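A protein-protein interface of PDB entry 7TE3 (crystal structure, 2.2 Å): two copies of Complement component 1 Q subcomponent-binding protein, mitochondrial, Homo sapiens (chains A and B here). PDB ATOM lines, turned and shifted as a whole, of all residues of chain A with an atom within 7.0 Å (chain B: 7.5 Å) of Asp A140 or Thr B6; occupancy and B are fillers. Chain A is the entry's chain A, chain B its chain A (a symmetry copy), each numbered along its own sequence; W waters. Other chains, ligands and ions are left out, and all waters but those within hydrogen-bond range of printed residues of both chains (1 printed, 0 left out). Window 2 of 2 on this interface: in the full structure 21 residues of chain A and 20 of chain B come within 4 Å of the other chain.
The side-chain carboxylate of Asp B9 is in salt-bridge range of the guanidinium group of Arg A141 (2.7 Å).
Water W1 bridges the side-chain carboxylate (OD1) of Asp B9 and the side-chain carboxylate (OD2) of Asp A140.
The side-chain carboxylate (OE1) of Glu A57 lies within salt-bridge range of the guanidinium group (NE) of Arg A141 (2.7 Å). O of Phe A137 is in hydrogen-bond range of NH1 of Arg A141 (3.2 Å).
No position is printed for both chains.
Printed residues of chain A that touch a printed residue of chain B: His A133, Phe A137, Asp A140 and Arg A141. Hydrophobic or aromatic side chains of chain A that line the printed part of chain B: His A133 and Phe A137. Printed residues of chain B that touch a printed residue of chain A: Thr B6, Gly B8, Asp B9 and Phe B12. Along chain B the printed residues that touch a printed residue of chain A span positions 6 to 12. Among the printed residues, Asp or Glu carboxylates within 4 Å of a Lys or Arg side-chain nitrogen of the other chain: Arg A141 with Asp B9.
Of chain B, only Thr B6 (3.3 Å) and Gly B8 (3.9 Å) come within 4 Å of Asp A140. Thr B6 touches just one residue of chain A: Asp A140. No residue of chain B comes within 4 Å of Ala A139. Printed residues of chain A within 4 Å of Gly B8: Asp A140. Printed residues of chain B within 4 Å of Phe A137: Asp B9. Printed residues of chain A within 4 Å of Asp B9: Phe A137 and Arg A141. Val A54 touches none of the printed residues of chain B. Asp A136 touches none of the printed residues of chain B. The nearest printed residue of chain B that does not touch Arg A141 is Thr B6 (5.4 Å).
Among the printed residues, pairs that only touch across the chains: His A133 with Phe B12 (3.6 Å), Phe A137 with Asp B9 (3.6 Å), Asp A140 with Thr B6 (3.3 Å) and Asp A140 with Gly B8 (3.9 Å).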
ATOM      1  N   ARG A  52      23.888   5.817  -2.824  1.00  0.00           N
ATOM      2  CA  ARG A  52      23.025   5.112  -1.898  1.00  0.00           C
ATOM      3  C   ARG A  52      22.039   4.327  -2.745  1.00  0.00           C
ATOM      4  O   ARG A  52      21.437   4.895  -3.662  1.00  0.00           O
ATOM      5  CB  ARG A  52      22.310   6.120  -0.990  1.00  0.00           C
ATOM      6  CG  ARG A  52      21.770   5.589   0.303  1.00  0.00           C
ATOM      7  CD  ARG A  52      21.241   6.743   1.176  1.00  0.00           C
ATOM      8  NE  ARG A  52      20.168   6.287   2.050  1.00  0.00           N
ATOM      9  CZ  ARG A  52      19.633   7.002   3.030  1.00  0.00           C
ATOM     10  NH1 ARG A  52      20.047   8.230   3.301  1.00  0.00           N
ATOM     11  NH2 ARG A  52      18.643   6.476   3.747  1.00  0.00           N
ATOM     12  N   VAL A  54      18.678   2.111  -1.928  1.00  0.00           N
ATOM     13  CA  VAL A  54      17.785   1.867  -0.800  1.00  0.00           C
ATOM     14  C   VAL A  54      16.680   0.884  -1.173  1.00  0.00           C
ATOM     15  O   VAL A  54      16.804  -0.325  -0.934  1.00  0.00           O
ATOM     16  CB  VAL A  54      17.190   3.182  -0.271  1.00  0.00           C
ATOM     17  CG1 VAL A  54      16.372   2.922   0.982  1.00  0.00           C
ATOM     18  CG2 VAL A  54      18.294   4.175   0.031  1.00  0.00           C
ATOM     19  N   GLU A  57      15.776   2.027  -5.531  1.00  0.00           N
ATOM     20  CA  GLU A  57      16.233   3.347  -5.933  1.00  0.00           C
ATOM     21  C   GLU A  57      17.735   3.458  -5.759  1.00  0.00           C
ATOM     22  O   GLU A  57      18.296   2.974  -4.773  1.00  0.00           O
ATOM     23  CB  GLU A  57      15.533   4.460  -5.128  1.00  0.00           C
ATOM     24  CG  GLU A  57      14.327   5.018  -5.844  1.00  0.00           C
ATOM     25  CD  GLU A  57      13.612   6.110  -5.076  1.00  0.00           C
ATOM     26  OE1 GLU A  57      14.213   6.711  -4.161  1.00  0.00           O
ATOM     27  OE2 GLU A  57      12.439   6.365  -5.403  1.00  0.00           O
ATOM     28  N   HIS A 133       7.026  20.135  -1.540  1.00  0.00           N
ATOM     29  CA  HIS A 133       6.950  18.703  -1.843  1.00  0.00           C
ATOM     30  C   HIS A 133       8.255  18.188  -2.449  1.00  0.00           C
ATOM     31  O   HIS A 133       8.671  17.057  -2.174  1.00  0.00           O
ATOM     32  CB  HIS A 133       5.788  18.425  -2.793  1.00  0.00           C
ATOM     33  CG  HIS A 133       4.458  18.334  -2.121  1.00  0.00           C
ATOM     34  ND1 HIS A 133       4.150  17.335  -1.224  1.00  0.00           N
ATOM     35  CD2 HIS A 133       3.341  19.092  -2.236  1.00  0.00           C
ATOM     36  CE1 HIS A 133       2.909  17.487  -0.804  1.00  0.00           C
ATOM     37  NE2 HIS A 133       2.394  18.545  -1.404  1.00  0.00           N
ATOM     38  N   MET A 135      11.245  19.449  -1.835  1.00  0.00           N
ATOM     39  CA  MET A 135      12.160  19.373  -0.703  1.00  0.00           C
ATOM     40  C   MET A 135      11.891  18.125   0.134  1.00  0.00           C
ATOM     41  O   MET A 135      12.833  17.434   0.544  1.00  0.00           O
ATOM     42  CB  MET A 135      12.052  20.635   0.164  1.00  0.00           C
ATOM     43  CG  MET A 135      12.600  21.919  -0.482  1.00  0.00           C
ATOM     44  SD  MET A 135      14.395  21.894  -0.797  1.00  0.00           S
ATOM     45  CE  MET A 135      15.005  22.171   0.867  1.00  0.00           C
ATOM     46  N   ASP A 136      10.609  17.815   0.398  1.00  0.00           N
ATOM     47  CA  ASP A 136      10.282  16.590   1.132  1.00  0.00           C
ATOM     48  C   ASP A 136      10.711  15.336   0.362  1.00  0.00           C
ATOM     49  O   ASP A 136      11.180  14.361   0.958  1.00  0.00           O
ATOM     50  CB  ASP A 136       8.788  16.534   1.439  1.00  0.00           C
ATOM     51  CG  ASP A 136       8.361  17.542   2.498  1.00  0.00           C
ATOM     52  OD1 ASP A 136       9.231  18.230   3.074  1.00  0.00           O
ATOM     53  OD2 ASP A 136       7.145  17.648   2.753  1.00  0.00           O
ATOM     54  N   PHE A 137      10.539  15.336  -0.960  1.00  0.00           N
ATOM     55  CA  PHE A 137      10.993  14.208  -1.776  1.00  0.00           C
ATOM     56  C   PHE A 137      12.485  13.951  -1.576  1.00  0.00           C
ATOM     57  O   PHE A 137      12.911  12.804  -1.393  1.00  0.00           O
ATOM     58  CB  PHE A 137      10.671  14.478  -3.250  1.00  0.00           C
ATOM     59  CG  PHE A 137      11.092  13.369  -4.196  1.00  0.00           C
ATOM     60  CD1 PHE A 137      10.286  12.263  -4.396  1.00  0.00           C
ATOM     61  CD2 PHE A 137      12.282  13.450  -4.899  1.00  0.00           C
ATOM     62  CE1 PHE A 137      10.666  11.256  -5.272  1.00  0.00           C
ATOM     63  CE2 PHE A 137      12.660  12.445  -5.769  1.00  0.00           C
ATOM     64  CZ  PHE A 137      11.858  11.354  -5.957  1.00  0.00           C
ATOM     65  N   LEU A 138      13.293  15.015  -1.582  1.00  0.00           N
ATOM     66  CA  LEU A 138      14.725  14.879  -1.314  1.00  0.00           C
ATOM     67  C   LEU A 138      14.981  14.422   0.116  1.00  0.00           C
ATOM     68  O   LEU A 138      15.798  13.524   0.356  1.00  0.00           O
ATOM     69  CB  LEU A 138      15.444  16.205  -1.580  1.00  0.00           C
ATOM     70  CG  LEU A 138      15.734  16.607  -3.039  1.00  0.00           C
ATOM     71  CD1 LEU A 138      16.494  17.935  -3.091  1.00  0.00           C
ATOM     72  CD2 LEU A 138      16.534  15.526  -3.744  1.00  0.00           C
ATOM     73  N   ALA A 139      14.313  15.050   1.088  1.00  0.00           N
ATOM     74  CA  ALA A 139      14.547  14.699   2.485  1.00  0.00           C
ATOM     75  C   ALA A 139      14.270  13.220   2.745  1.00  0.00           C
ATOM     76  O   ALA A 139      15.006  12.561   3.487  1.00  0.00           O
ATOM     77  CB  ALA A 139      13.686  15.580   3.396  1.00  0.00           C
ATOM     78  N   ASP A 140      13.218  12.678   2.130  1.00  0.00           N
ATOM     79  CA  ASP A 140      12.897  11.263   2.303  1.00  0.00           C
ATOM     80  C   ASP A 140      14.021  10.366   1.804  1.00  0.00           C
ATOM     81  O   ASP A 140      14.173   9.233   2.275  1.00  0.00           O
ATOM     82  CB  ASP A 140      11.597  10.927   1.571  1.00  0.00           C
ATOM     83  CG  ASP A 140      10.363  11.343   2.347  1.00  0.00           C
ATOM     84  OD1 ASP A 140      10.482  11.582   3.565  1.00  0.00           O
ATOM     85  OD2 ASP A 140       9.273  11.406   1.743  1.00  0.00           O
ATOM     86  N   ARG A 141      14.817  10.856   0.863  1.00  0.00           N
ATOM     87  CA  ARG A 141      15.918  10.097   0.299  1.00  0.00           C
ATOM     88  C   ARG A 141      17.258  10.429   0.943  1.00  0.00           C
ATOM     89  O   ARG A 141      18.299  10.039   0.412  1.00  0.00           O
ATOM     90  CB  ARG A 141      15.951  10.311  -1.210  1.00  0.00           C
ATOM     91  CG  ARG A 141      14.973   9.365  -1.896  1.00  0.00           C
ATOM     92  CD  ARG A 141      14.166   9.999  -3.011  1.00  0.00           C
ATOM     93  NE  ARG A 141      13.100   9.098  -3.451  1.00  0.00           N
ATOM     94  CZ  ARG A 141      11.843   9.140  -3.020  1.00  0.00           C
ATOM     95  NH1 ARG A 141      11.442  10.057  -2.152  1.00  0.00           N
ATOM     96  NH2 ARG A 141      10.966   8.245  -3.478  1.00  0.00           N
ATOM     97  N   GLY A 142      17.256  11.112   2.082  1.00  0.00           N
ATOM     98  CA  GLY A 142      18.467  11.419   2.805  1.00  0.00           C
ATOM     99  C   GLY A 142      19.061  12.783   2.532  1.00  0.00           C
ATOM    100  O   GLY A 142      19.956  13.203   3.273  1.00  0.00           O
ATOM    101  N   VAL A 143      18.598  13.493   1.505  1.00  0.00           N
ATOM    102  CA  VAL A 143      19.173  14.792   1.146  1.00  0.00           C
ATOM    103  C   VAL A 143      18.355  15.847   1.894  1.00  0.00           C
ATOM    104  O   VAL A 143      17.389  16.393   1.379  1.00  0.00           O
ATOM    105  CB  VAL A 143      19.187  15.030  -0.358  1.00  0.00           C
ATOM    106  CG1 VAL A 143      19.818  16.384  -0.671  1.00  0.00           C
ATOM    107  CG2 VAL A 143      19.938  13.896  -1.087  1.00  0.00           C
ATOM    108  N   ASP A 144      18.767  16.123   3.120  1.00  0.00           N
ATOM    109  CA  ASP A 144      18.128  17.071   4.024  1.00  0.00           C
ATOM    110  C   ASP A 144      19.114  18.192   4.336  1.00  0.00           C
ATOM    111  O   ASP A 144      20.217  18.245   3.785  1.00  0.00           O
ATOM    112  CB  ASP A 144      17.656  16.363   5.299  1.00  0.00           C
ATOM    113  CG  ASP A 144      18.709  15.414   5.870  1.00  0.00           C
ATOM    114  OD1 ASP A 144      19.901  15.790   5.882  1.00  0.00           O
ATOM    115  OD2 ASP A 144      18.352  14.296   6.326  1.00  0.00           O
ATOM    116  N   THR B   6       6.242   5.239   0.853  1.00  0.00           N
ATOM    117  CA  THR B   6       6.479   6.386   1.722  1.00  0.00           C
ATOM    118  C   THR B   6       5.223   7.246   1.846  1.00  0.00           C
ATOM    119  O   THR B   6       4.495   7.431   0.867  1.00  0.00           O
ATOM    120  CB  THR B   6       7.641   7.261   1.203  1.00  0.00           C
ATOM    121  OG1 THR B   6       8.838   6.477   1.137  1.00  0.00           O
ATOM    122  CG2 THR B   6       7.876   8.465   2.116  1.00  0.00           C
ATOM    123  N   ASP B   7       4.975   7.762   3.055  1.00  0.00           N
ATOM    124  CA  ASP B   7       3.882   8.712   3.257  1.00  0.00           C
ATOM    125  C   ASP B   7       4.017   9.915   2.329  1.00  0.00           C
ATOM    126  O   ASP B   7       3.059  10.300   1.647  1.00  0.00           O
ATOM    127  CB  ASP B   7       3.848   9.172   4.714  1.00  0.00           C
ATOM    128  CG  ASP B   7       3.806   8.015   5.691  1.00  0.00           C
ATOM    129  OD1 ASP B   7       3.362   6.914   5.296  1.00  0.00           O
ATOM    130  OD2 ASP B   7       4.209   8.216   6.859  1.00  0.00           O
ATOM    131  N   GLY B   8       5.208  10.521   2.295  1.00  0.00           N
ATOM    132  CA  GLY B   8       5.395  11.713   1.492  1.00  0.00           C
ATOM    133  C   GLY B   8       5.138  11.461   0.023  1.00  0.00           C
ATOM    134  O   GLY B   8       4.495  12.269  -0.650  1.00  0.00           O
ATOM    135  N   ASP B   9       5.607  10.318  -0.482  1.00  0.00           N
ATOM    136  CA  ASP B   9       5.513  10.031  -1.910  1.00  0.00           C
ATOM    137  C   ASP B   9       4.063  10.005  -2.377  1.00  0.00           C
ATOM    138  O   ASP B   9       3.698  10.674  -3.353  1.00  0.00           O
ATOM    139  CB  ASP B   9       6.211   8.703  -2.223  1.00  0.00           C
ATOM    140  CG  ASP B   9       7.691   8.874  -2.569  1.00  0.00           C
ATOM    141  OD1 ASP B   9       8.215  10.014  -2.526  1.00  0.00           O
ATOM    142  OD2 ASP B   9       8.338   7.861  -2.897  1.00  0.00           O
ATOM    143  N   LYS B  10       3.214   9.240  -1.694  1.00  0.00           N
ATOM    144  CA  LYS B  10       1.842   9.110  -2.167  1.00  0.00           C
ATOM    145  C   LYS B  10       1.057  10.397  -1.958  1.00  0.00           C
ATOM    146  O   LYS B  10       0.129  10.674  -2.721  1.00  0.00           O
ATOM    147  CB  LYS B  10       1.160   7.915  -1.497  1.00  0.00           C
ATOM    148  CG  LYS B  10       1.539   7.696  -0.035  1.00  0.00           C
ATOM    149  CD  LYS B  10       1.444   6.208   0.346  1.00  0.00           C
ATOM    150  CE  LYS B  10       1.862   5.955   1.796  1.00  0.00           C
ATOM    151  NZ  LYS B  10       2.000   4.496   2.093  1.00  0.00           N
ATOM    152  N   ALA B  11       1.429  11.209  -0.961  1.00  0.00           N
ATOM    153  CA  ALA B  11       0.845  12.545  -0.834  1.00  0.00           C
ATOM    154  C   ALA B  11       1.300  13.464  -1.966  1.00  0.00           C
ATOM    155  O   ALA B  11       0.507  14.263  -2.481  1.00  0.00           O
ATOM    156  CB  ALA B  11       1.215  13.153   0.514  1.00  0.00           C
ATOM    157  N   PHE B  12       2.583  13.377  -2.335  1.00  0.00           N
ATOM    158  CA  PHE B  12       3.117  14.102  -3.486  1.00  0.00           C
ATOM    159  C   PHE B  12       2.401  13.688  -4.771  1.00  0.00           C
ATOM    160  O   PHE B  12       2.193  14.510  -5.669  1.00  0.00           O
ATOM    161  CB  PHE B  12       4.630  13.838  -3.578  1.00  0.00           C
ATOM    162  CG  PHE B  12       5.400  14.752  -4.525  1.00  0.00           C
ATOM    163  CD1 PHE B  12       4.814  15.855  -5.129  1.00  0.00           C
ATOM    164  CD2 PHE B  12       6.739  14.496  -4.793  1.00  0.00           C
ATOM    165  CE1 PHE B  12       5.543  16.689  -5.985  1.00  0.00           C
ATOM    166  CE2 PHE B  12       7.483  15.314  -5.658  1.00  0.00           C
ATOM    167  CZ  PHE B  12       6.881  16.417  -6.260  1.00  0.00           C
ATOM    168  N   GLN B 177       6.584   1.897  -8.363  1.00  0.00           N
ATOM    169  CA  GLN B 177       6.825   1.071  -7.158  1.00  0.00           C
ATOM    170  C   GLN B 177       5.707   1.205  -6.121  1.00  0.00           C
ATOM    171  O   GLN B 177       5.299   2.310  -5.758  1.00  0.00           O
ATOM    172  CB  GLN B 177       8.164   1.401  -6.501  1.00  0.00           C
ATOM    173  CG  GLN B 177       9.355   1.163  -7.386  1.00  0.00           C
ATOM    174  CD  GLN B 177      10.612   1.803  -6.843  1.00  0.00           C
ATOM    175  OE1 GLN B 177      10.583   2.477  -5.809  1.00  0.00           O
ATOM    176  NE2 GLN B 177      11.729   1.598  -7.536  1.00  0.00           N
ATOM    177  OXT GLN B 177       5.191   0.207  -5.607  1.00  0.00           O
HETATM  178  O   HOH W   1       8.523  12.279  -0.872  1.00  0.00           O
